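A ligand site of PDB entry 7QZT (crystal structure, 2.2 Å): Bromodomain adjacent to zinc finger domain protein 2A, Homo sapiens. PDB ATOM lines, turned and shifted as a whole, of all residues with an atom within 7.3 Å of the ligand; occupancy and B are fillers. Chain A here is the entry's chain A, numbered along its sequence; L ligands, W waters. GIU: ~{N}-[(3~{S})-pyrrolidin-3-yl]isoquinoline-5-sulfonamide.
Merely in contact with the ligand: Asn 80 (3.4 Å), Pro 24 (3.4 Å), Val 29 (3.5 Å), Trp 23 (3.5 Å), Val 34 (3.7 Å), Phe 79 (3.8 Å), Val 86 (3.8 Å) and Tyr 37 (3.8 Å). Hydrophobic or aromatic side chains within 4 Å of the ligand: Trp 23, Pro 24, Val 29, Val 34, Tyr 37, Phe 79 and Val 86. Of the 23 residues printed, 10 come within 4 Å of the ligand.
Water W2 bridges N14 of the ligand (2.8 Å) and OH of Tyr 37 (2.9 Å). Water W3 bridges N04 of the ligand and N of Asn 30. Water W1 lies within hydrogen-bond range of N of Glu 27 (2.9 Å), O of Trp 23 (3.0 Å), N of Leu 26 (3.1 Å), N08 of the ligand (3.4 Å) and O of Pro 24 (3.4 Å).
ND2 of Asn 80 is in hydrogen-bond range of O of Cys 76 (2.9 Å).
The backbone carbonyl oxygen of Pro 28 lies within hydrogen-bond range of a nitrogen (N08) of the ligand (3.0 Å). The backbone carbonyl oxygen (O) of Glu 27 is in hydrogen-bond range of a nitrogen (N08) of the ligand.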
ATOM      1  N   ALA A  22      21.120  29.546  -6.097  1.00  0.00           N
ATOM      2  CA  ALA A  22      20.891  29.170  -4.710  1.00  0.00           C
ATOM      3  C   ALA A  22      20.995  27.679  -4.501  1.00  0.00           C
ATOM      4  O   ALA A  22      21.035  27.247  -3.352  1.00  0.00           O
ATOM      5  CB  ALA A  22      19.506  29.636  -4.260  1.00  0.00           C
ATOM      6  N   TRP A  23      21.065  26.896  -5.570  1.00  0.00           N
ATOM      7  CA  TRP A  23      20.934  25.455  -5.428  1.00  0.00           C
ATOM      8  C   TRP A  23      21.920  24.797  -4.444  1.00  0.00           C
ATOM      9  O   TRP A  23      21.510  23.803  -3.826  1.00  0.00           O
ATOM     10  CB  TRP A  23      21.016  24.797  -6.810  1.00  0.00           C
ATOM     11  CG  TRP A  23      22.257  25.090  -7.527  1.00  0.00           C
ATOM     12  CD1 TRP A  23      22.466  26.092  -8.410  1.00  0.00           C
ATOM     13  CD2 TRP A  23      23.503  24.388  -7.420  1.00  0.00           C
ATOM     14  NE1 TRP A  23      23.764  26.057  -8.880  1.00  0.00           N
ATOM     15  CE2 TRP A  23      24.420  25.019  -8.280  1.00  0.00           C
ATOM     16  CE3 TRP A  23      23.938  23.280  -6.679  1.00  0.00           C
ATOM     17  CZ2 TRP A  23      25.748  24.584  -8.421  1.00  0.00           C
ATOM     18  CZ3 TRP A  23      25.250  22.850  -6.825  1.00  0.00           C
ATOM     19  CH2 TRP A  23      26.140  23.514  -7.687  1.00  0.00           C
ATOM     20  N   PRO A  24      23.153  25.265  -4.215  1.00  0.00           N
ATOM     21  CA  PRO A  24      23.994  24.562  -3.233  1.00  0.00           C
ATOM     22  C   PRO A  24      23.597  24.812  -1.789  1.00  0.00           C
ATOM     23  O   PRO A  24      24.078  24.090  -0.905  1.00  0.00           O
ATOM     24  CB  PRO A  24      25.408  25.114  -3.481  1.00  0.00           C
ATOM     25  CG  PRO A  24      25.324  25.905  -4.719  1.00  0.00           C
ATOM     26  CD  PRO A  24      23.903  26.373  -4.820  1.00  0.00           C
ATOM     27  N   PHE A  25      22.748  25.811  -1.529  1.00  0.00           N
ATOM     28  CA  PHE A  25      22.556  26.340  -0.186  1.00  0.00           C
ATOM     29  C   PHE A  25      21.122  26.227   0.293  1.00  0.00           C
ATOM     30  O   PHE A  25      20.801  26.760   1.374  1.00  0.00           O
ATOM     31  CB  PHE A  25      23.011  27.806  -0.125  1.00  0.00           C
ATOM     32  CG  PHE A  25      24.340  28.020  -0.774  1.00  0.00           C
ATOM     33  CD1 PHE A  25      25.481  27.446  -0.245  1.00  0.00           C
ATOM     34  CD2 PHE A  25      24.444  28.732  -1.946  1.00  0.00           C
ATOM     35  CE1 PHE A  25      26.714  27.603  -0.865  1.00  0.00           C
ATOM     36  CE2 PHE A  25      25.688  28.897  -2.575  1.00  0.00           C
ATOM     37  CZ  PHE A  25      26.809  28.326  -2.037  1.00  0.00           C
ATOM     38  N   LEU A  26      20.263  25.525  -0.444  1.00  0.00           N
ATOM     39  CA  LEU A  26      18.849  25.484  -0.088  1.00  0.00           C
ATOM     40  C   LEU A  26      18.595  24.509   1.038  1.00  0.00           C
ATOM     41  O   LEU A  26      17.723  24.782   1.865  1.00  0.00           O
ATOM     42  CB  LEU A  26      17.997  25.118  -1.301  1.00  0.00           C
ATOM     43  CG  LEU A  26      17.941  26.150  -2.421  1.00  0.00           C
ATOM     44  CD1 LEU A  26      17.601  25.456  -3.712  1.00  0.00           C
ATOM     45  CD2 LEU A  26      16.921  27.243  -2.102  1.00  0.00           C
ATOM     46  N   GLU A  27      19.342  23.414   1.104  1.00  0.00           N
ATOM     47  CA  GLU A  27      19.227  22.352   2.115  1.00  0.00           C
ATOM     48  C   GLU A  27      20.577  22.032   2.778  1.00  0.00           C
ATOM     49  O   GLU A  27      21.628  22.187   2.152  1.00  0.00           O
ATOM     50  CB  GLU A  27      18.691  21.061   1.471  1.00  0.00           C
ATOM     51  CG  GLU A  27      17.317  21.216   0.823  1.00  0.00           C
ATOM     52  CD  GLU A  27      16.222  21.449   1.852  1.00  0.00           C
ATOM     53  OE1 GLU A  27      16.413  21.043   3.024  1.00  0.00           O
ATOM     54  OE2 GLU A  27      15.171  22.046   1.508  1.00  0.00           O
ATOM     55  N   PRO A  28      20.555  21.597   4.043  1.00  0.00           N
ATOM     56  CA  PRO A  28      21.829  21.261   4.713  1.00  0.00           C
ATOM     57  C   PRO A  28      22.707  20.334   3.879  1.00  0.00           C
ATOM     58  O   PRO A  28      22.227  19.518   3.101  1.00  0.00           O
ATOM     59  CB  PRO A  28      21.384  20.592   6.015  1.00  0.00           C
ATOM     60  CG  PRO A  28      20.110  21.238   6.324  1.00  0.00           C
ATOM     61  CD  PRO A  28      19.421  21.479   4.962  1.00  0.00           C
ATOM     62  N   VAL A  29      24.019  20.469   4.069  1.00  0.00           N
ATOM     63  CA  VAL A  29      24.938  19.568   3.379  1.00  0.00           C
ATOM     64  C   VAL A  29      24.801  18.186   4.002  1.00  0.00           C
ATOM     65  O   VAL A  29      24.761  18.033   5.223  1.00  0.00           O
ATOM     66  CB  VAL A  29      26.380  20.076   3.455  1.00  0.00           C
ATOM     67  CG1 VAL A  29      27.322  19.025   2.955  1.00  0.00           C
ATOM     68  CG2 VAL A  29      26.548  21.320   2.581  1.00  0.00           C
ATOM     69  N   ASN A  30      24.678  17.180   3.158  1.00  0.00           N
ATOM     70  CA  ASN A  30      24.619  15.837   3.710  1.00  0.00           C
ATOM     71  C   ASN A  30      26.014  15.290   3.900  1.00  0.00           C
ATOM     72  O   ASN A  30      26.660  14.877   2.927  1.00  0.00           O
ATOM     73  CB  ASN A  30      23.823  14.908   2.799  1.00  0.00           C
ATOM     74  CG  ASN A  30      23.656  13.518   3.409  1.00  0.00           C
ATOM     75  OD1 ASN A  30      24.369  13.146   4.342  1.00  0.00           O
ATOM     76  ND2 ASN A  30      22.707  12.756   2.871  1.00  0.00           N
ATOM     77  N   LEU A  33      27.315  12.230   2.214  1.00  0.00           N
ATOM     78  CA  LEU A  33      27.580  12.304   0.788  1.00  0.00           C
ATOM     79  C   LEU A  33      28.739  13.207   0.433  1.00  0.00           C
ATOM     80  O   LEU A  33      29.270  13.093  -0.668  1.00  0.00           O
ATOM     81  CB  LEU A  33      26.339  12.825   0.033  1.00  0.00           C
ATOM     82  CG  LEU A  33      25.068  11.984   0.238  1.00  0.00           C
ATOM     83  CD1 LEU A  33      23.792  12.791  -0.103  1.00  0.00           C
ATOM     84  CD2 LEU A  33      25.157  10.723  -0.593  1.00  0.00           C
ATOM     85  N   VAL A  34      29.135  14.118   1.317  1.00  0.00           N
ATOM     86  CA  VAL A  34      30.223  15.051   1.043  1.00  0.00           C
ATOM     87  C   VAL A  34      31.389  14.655   1.945  1.00  0.00           C
ATOM     88  O   VAL A  34      31.415  15.002   3.127  1.00  0.00           O
ATOM     89  CB  VAL A  34      29.804  16.501   1.279  1.00  0.00           C
ATOM     90  CG1 VAL A  34      30.938  17.437   0.891  1.00  0.00           C
ATOM     91  CG2 VAL A  34      28.577  16.810   0.466  1.00  0.00           C
ATOM     92  N   SER A  35      32.346  13.930   1.378  1.00  0.00           N
ATOM     93  CA  SER A  35      33.459  13.456   2.189  1.00  0.00           C
ATOM     94  C   SER A  35      34.261  14.637   2.729  1.00  0.00           C
ATOM     95  O   SER A  35      34.569  15.595   2.019  1.00  0.00           O
ATOM     96  CB  SER A  35      34.359  12.547   1.367  1.00  0.00           C
ATOM     97  OG  SER A  35      35.329  11.959   2.223  1.00  0.00           O
ATOM     98  N   TYR A  37      33.234  16.851   4.916  1.00  0.00           N
ATOM     99  CA  TYR A  37      32.483  18.049   5.288  1.00  0.00           C
ATOM    100  C   TYR A  37      32.349  18.162   6.805  1.00  0.00           C
ATOM    101  O   TYR A  37      32.572  19.239   7.386  1.00  0.00           O
ATOM    102  CB  TYR A  37      31.094  18.044   4.630  1.00  0.00           C
ATOM    103  CG  TYR A  37      30.506  19.428   4.604  1.00  0.00           C
ATOM    104  CD1 TYR A  37      30.925  20.359   3.659  1.00  0.00           C
ATOM    105  CD2 TYR A  37      29.578  19.820   5.552  1.00  0.00           C
ATOM    106  CE1 TYR A  37      30.421  21.658   3.668  1.00  0.00           C
ATOM    107  CE2 TYR A  37      29.057  21.124   5.556  1.00  0.00           C
ATOM    108  CZ  TYR A  37      29.490  22.020   4.616  1.00  0.00           C
ATOM    109  OH  TYR A  37      28.964  23.301   4.613  1.00  0.00           O
ATOM    110  N   ILE A  41      33.873  21.779   8.533  1.00  0.00           N
ATOM    111  CA  ILE A  41      32.882  22.840   8.724  1.00  0.00           C
ATOM    112  C   ILE A  41      32.291  22.691  10.129  1.00  0.00           C
ATOM    113  O   ILE A  41      31.417  21.838  10.361  1.00  0.00           O
ATOM    114  CB  ILE A  41      31.794  22.795   7.643  1.00  0.00           C
ATOM    115  CG1 ILE A  41      32.381  23.219   6.283  1.00  0.00           C
ATOM    116  CG2 ILE A  41      30.619  23.672   8.010  1.00  0.00           C
ATOM    117  CD1 ILE A  41      33.360  24.402   6.380  1.00  0.00           C
ATOM    118  N   MET A  45      25.428  25.830   7.974  1.00  0.00           N
ATOM    119  CA  MET A  45      24.272  26.700   7.908  1.00  0.00           C
ATOM    120  C   MET A  45      23.782  26.695   6.470  1.00  0.00           C
ATOM    121  O   MET A  45      24.584  26.550   5.546  1.00  0.00           O
ATOM    122  CB  MET A  45      24.608  28.126   8.369  1.00  0.00           C
ATOM    123  CG  MET A  45      23.443  29.111   8.348  1.00  0.00           C
ATOM    124  SD  MET A  45      22.111  28.597   9.436  1.00  0.00           S
ATOM    125  CE  MET A  45      22.966  28.134  10.917  1.00  0.00           C
ATOM    126  N   ASP A  46      22.467  26.851   6.299  1.00  0.00           N
ATOM    127  CA  ASP A  46      21.848  26.814   4.984  1.00  0.00           C
ATOM    128  C   ASP A  46      20.562  27.651   5.023  1.00  0.00           C
ATOM    129  O   ASP A  46      20.090  28.067   6.092  1.00  0.00           O
ATOM    130  CB  ASP A  46      21.542  25.379   4.562  1.00  0.00           C
ATOM    131  CG  ASP A  46      20.512  24.733   5.469  1.00  0.00           C
ATOM    132  OD1 ASP A  46      20.855  24.339   6.607  1.00  0.00           O
ATOM    133  OD2 ASP A  46      19.346  24.665   5.070  1.00  0.00           O
ATOM    134  N   VAL A  72      26.925  30.944   5.909  1.00  0.00           N
ATOM    135  CA  VAL A  72      26.704  30.134   4.712  1.00  0.00           C
ATOM    136  C   VAL A  72      27.856  30.317   3.737  1.00  0.00           C
ATOM    137  O   VAL A  72      28.520  29.339   3.336  1.00  0.00           O
ATOM    138  CB  VAL A  72      25.341  30.482   4.081  1.00  0.00           C
ATOM    139  CG1 VAL A  72      25.133  29.734   2.841  1.00  0.00           C
ATOM    140  CG2 VAL A  72      24.227  30.154   5.030  1.00  0.00           C
ATOM    141  N   ASN A  75      31.365  29.356   5.134  1.00  0.00           N
ATOM    142  CA  ASN A  75      31.493  27.914   4.994  1.00  0.00           C
ATOM    143  C   ASN A  75      31.750  27.530   3.545  1.00  0.00           C
ATOM    144  O   ASN A  75      32.569  26.651   3.255  1.00  0.00           O
ATOM    145  CB  ASN A  75      30.245  27.197   5.504  1.00  0.00           C
ATOM    146  CG  ASN A  75      30.180  27.163   6.998  1.00  0.00           C
ATOM    147  OD1 ASN A  75      31.205  26.999   7.669  1.00  0.00           O
ATOM    148  ND2 ASN A  75      29.003  27.340   7.545  1.00  0.00           N
ATOM    149  N   CYS A  76      31.054  28.192   2.623  1.00  0.00           N
ATOM    150  CA  CYS A  76      31.193  27.817   1.218  1.00  0.00           C
ATOM    151  C   CYS A  76      32.623  28.017   0.742  1.00  0.00           C
ATOM    152  O   CYS A  76      33.160  27.167   0.015  1.00  0.00           O
ATOM    153  CB  CYS A  76      30.241  28.631   0.366  1.00  0.00           C
ATOM    154  SG  CYS A  76      30.485  28.183  -1.317  1.00  0.00           S
ATOM    155  N   PHE A  79      35.052  25.296   2.391  1.00  0.00           N
ATOM    156  CA  PHE A  79      35.035  23.937   1.900  1.00  0.00           C
ATOM    157  C   PHE A  79      35.258  23.824   0.400  1.00  0.00           C
ATOM    158  O   PHE A  79      35.817  22.810  -0.063  1.00  0.00           O
ATOM    159  CB  PHE A  79      33.718  23.240   2.220  1.00  0.00           C
ATOM    160  CG  PHE A  79      33.777  21.786   1.943  1.00  0.00           C
ATOM    161  CD1 PHE A  79      34.388  20.934   2.846  1.00  0.00           C
ATOM    162  CD2 PHE A  79      33.303  21.282   0.753  1.00  0.00           C
ATOM    163  CE1 PHE A  79      34.476  19.597   2.591  1.00  0.00           C
ATOM    164  CE2 PHE A  79      33.389  19.941   0.481  1.00  0.00           C
ATOM    165  CZ  PHE A  79      33.968  19.093   1.411  1.00  0.00           C
ATOM    166  N   ASN A  80      34.802  24.784  -0.382  1.00  0.00           N
ATOM    167  CA  ASN A  80      34.818  24.652  -1.839  1.00  0.00           C
ATOM    168  C   ASN A  80      35.844  25.582  -2.460  1.00  0.00           C
ATOM    169  O   ASN A  80      35.982  26.732  -2.041  1.00  0.00           O
ATOM    170  CB  ASN A  80      33.448  24.943  -2.424  1.00  0.00           C
ATOM    171  CG  ASN A  80      32.394  24.129  -1.779  1.00  0.00           C
ATOM    172  OD1 ASN A  80      32.122  23.005  -2.203  1.00  0.00           O
ATOM    173  ND2 ASN A  80      31.803  24.658  -0.721  1.00  0.00           N
ATOM    174  N   VAL A  86      30.195  24.630  -6.889  1.00  0.00           N
ATOM    175  CA  VAL A  86      29.575  25.164  -5.687  1.00  0.00           C
ATOM    176  C   VAL A  86      30.250  26.459  -5.299  1.00  0.00           C
ATOM    177  O   VAL A  86      29.567  27.429  -4.930  1.00  0.00           O
ATOM    178  CB  VAL A  86      29.633  24.125  -4.561  1.00  0.00           C
ATOM    179  CG1 VAL A  86      29.209  24.756  -3.218  1.00  0.00           C
ATOM    180  CG2 VAL A  86      28.747  22.931  -4.957  1.00  0.00           C
ATOM    181  N   GLY A  87      31.578  26.486  -5.382  1.00  0.00           N
ATOM    182  CA  GLY A  87      32.362  27.698  -5.212  1.00  0.00           C
ATOM    183  C   GLY A  87      31.855  28.860  -6.036  1.00  0.00           C
ATOM    184  O   GLY A  87      31.491  29.895  -5.466  1.00  0.00           O
HETATM  185  C05 GIU L   1      23.484  20.465  -1.776  1.00  0.00           C
HETATM  186  C06 GIU L   1      22.195  19.763  -2.209  1.00  0.00           C
HETATM  187  C07 GIU L   1      21.868  19.026  -1.140  1.00  0.00           C
HETATM  188  C09 GIU L   1      23.366  20.614  -0.214  1.00  0.00           C
HETATM  189  C10 GIU L   1      27.510  20.234  -2.410  1.00  0.00           C
HETATM  190  C11 GIU L   1      27.858  21.274  -1.484  1.00  0.00           C
HETATM  191  C12 GIU L   1      26.935  22.277  -1.096  1.00  0.00           C
HETATM  192  C13 GIU L   1      27.333  23.265  -0.179  1.00  0.00           C
HETATM  193  C15 GIU L   1      29.454  22.343   0.008  1.00  0.00           C
HETATM  194  C16 GIU L   1      29.095  21.310  -0.936  1.00  0.00           C
HETATM  195  C17 GIU L   1      30.046  20.331  -1.308  1.00  0.00           C
HETATM  196  C18 GIU L   1      29.689  19.322  -2.215  1.00  0.00           C
HETATM  197  C19 GIU L   1      28.422  19.278  -2.776  1.00  0.00           C
HETATM  198  N04 GIU L   1      24.638  19.593  -2.087  1.00  0.00           N
HETATM  199  N08 GIU L   1      22.373  19.848   0.172  1.00  0.00           N
HETATM  200  N14 GIU L   1      28.571  23.275   0.356  1.00  0.00           N
HETATM  201  O01 GIU L   1      25.983  19.492  -4.450  1.00  0.00           O
HETATM  202  O03 GIU L   1      25.461  21.505  -3.616  1.00  0.00           O
HETATM  203  S02 GIU L   1      25.859  20.181  -3.168  1.00  0.00           S
HETATM  204  O   HOH W   1      21.034  22.645  -1.136  1.00  0.00           O
HETATM  205  O   HOH W   2      29.495  24.984   2.347  1.00  0.00           O
HETATM  206  O   HOH W   3      24.596  17.270  -0.018  1.00  0.00           O
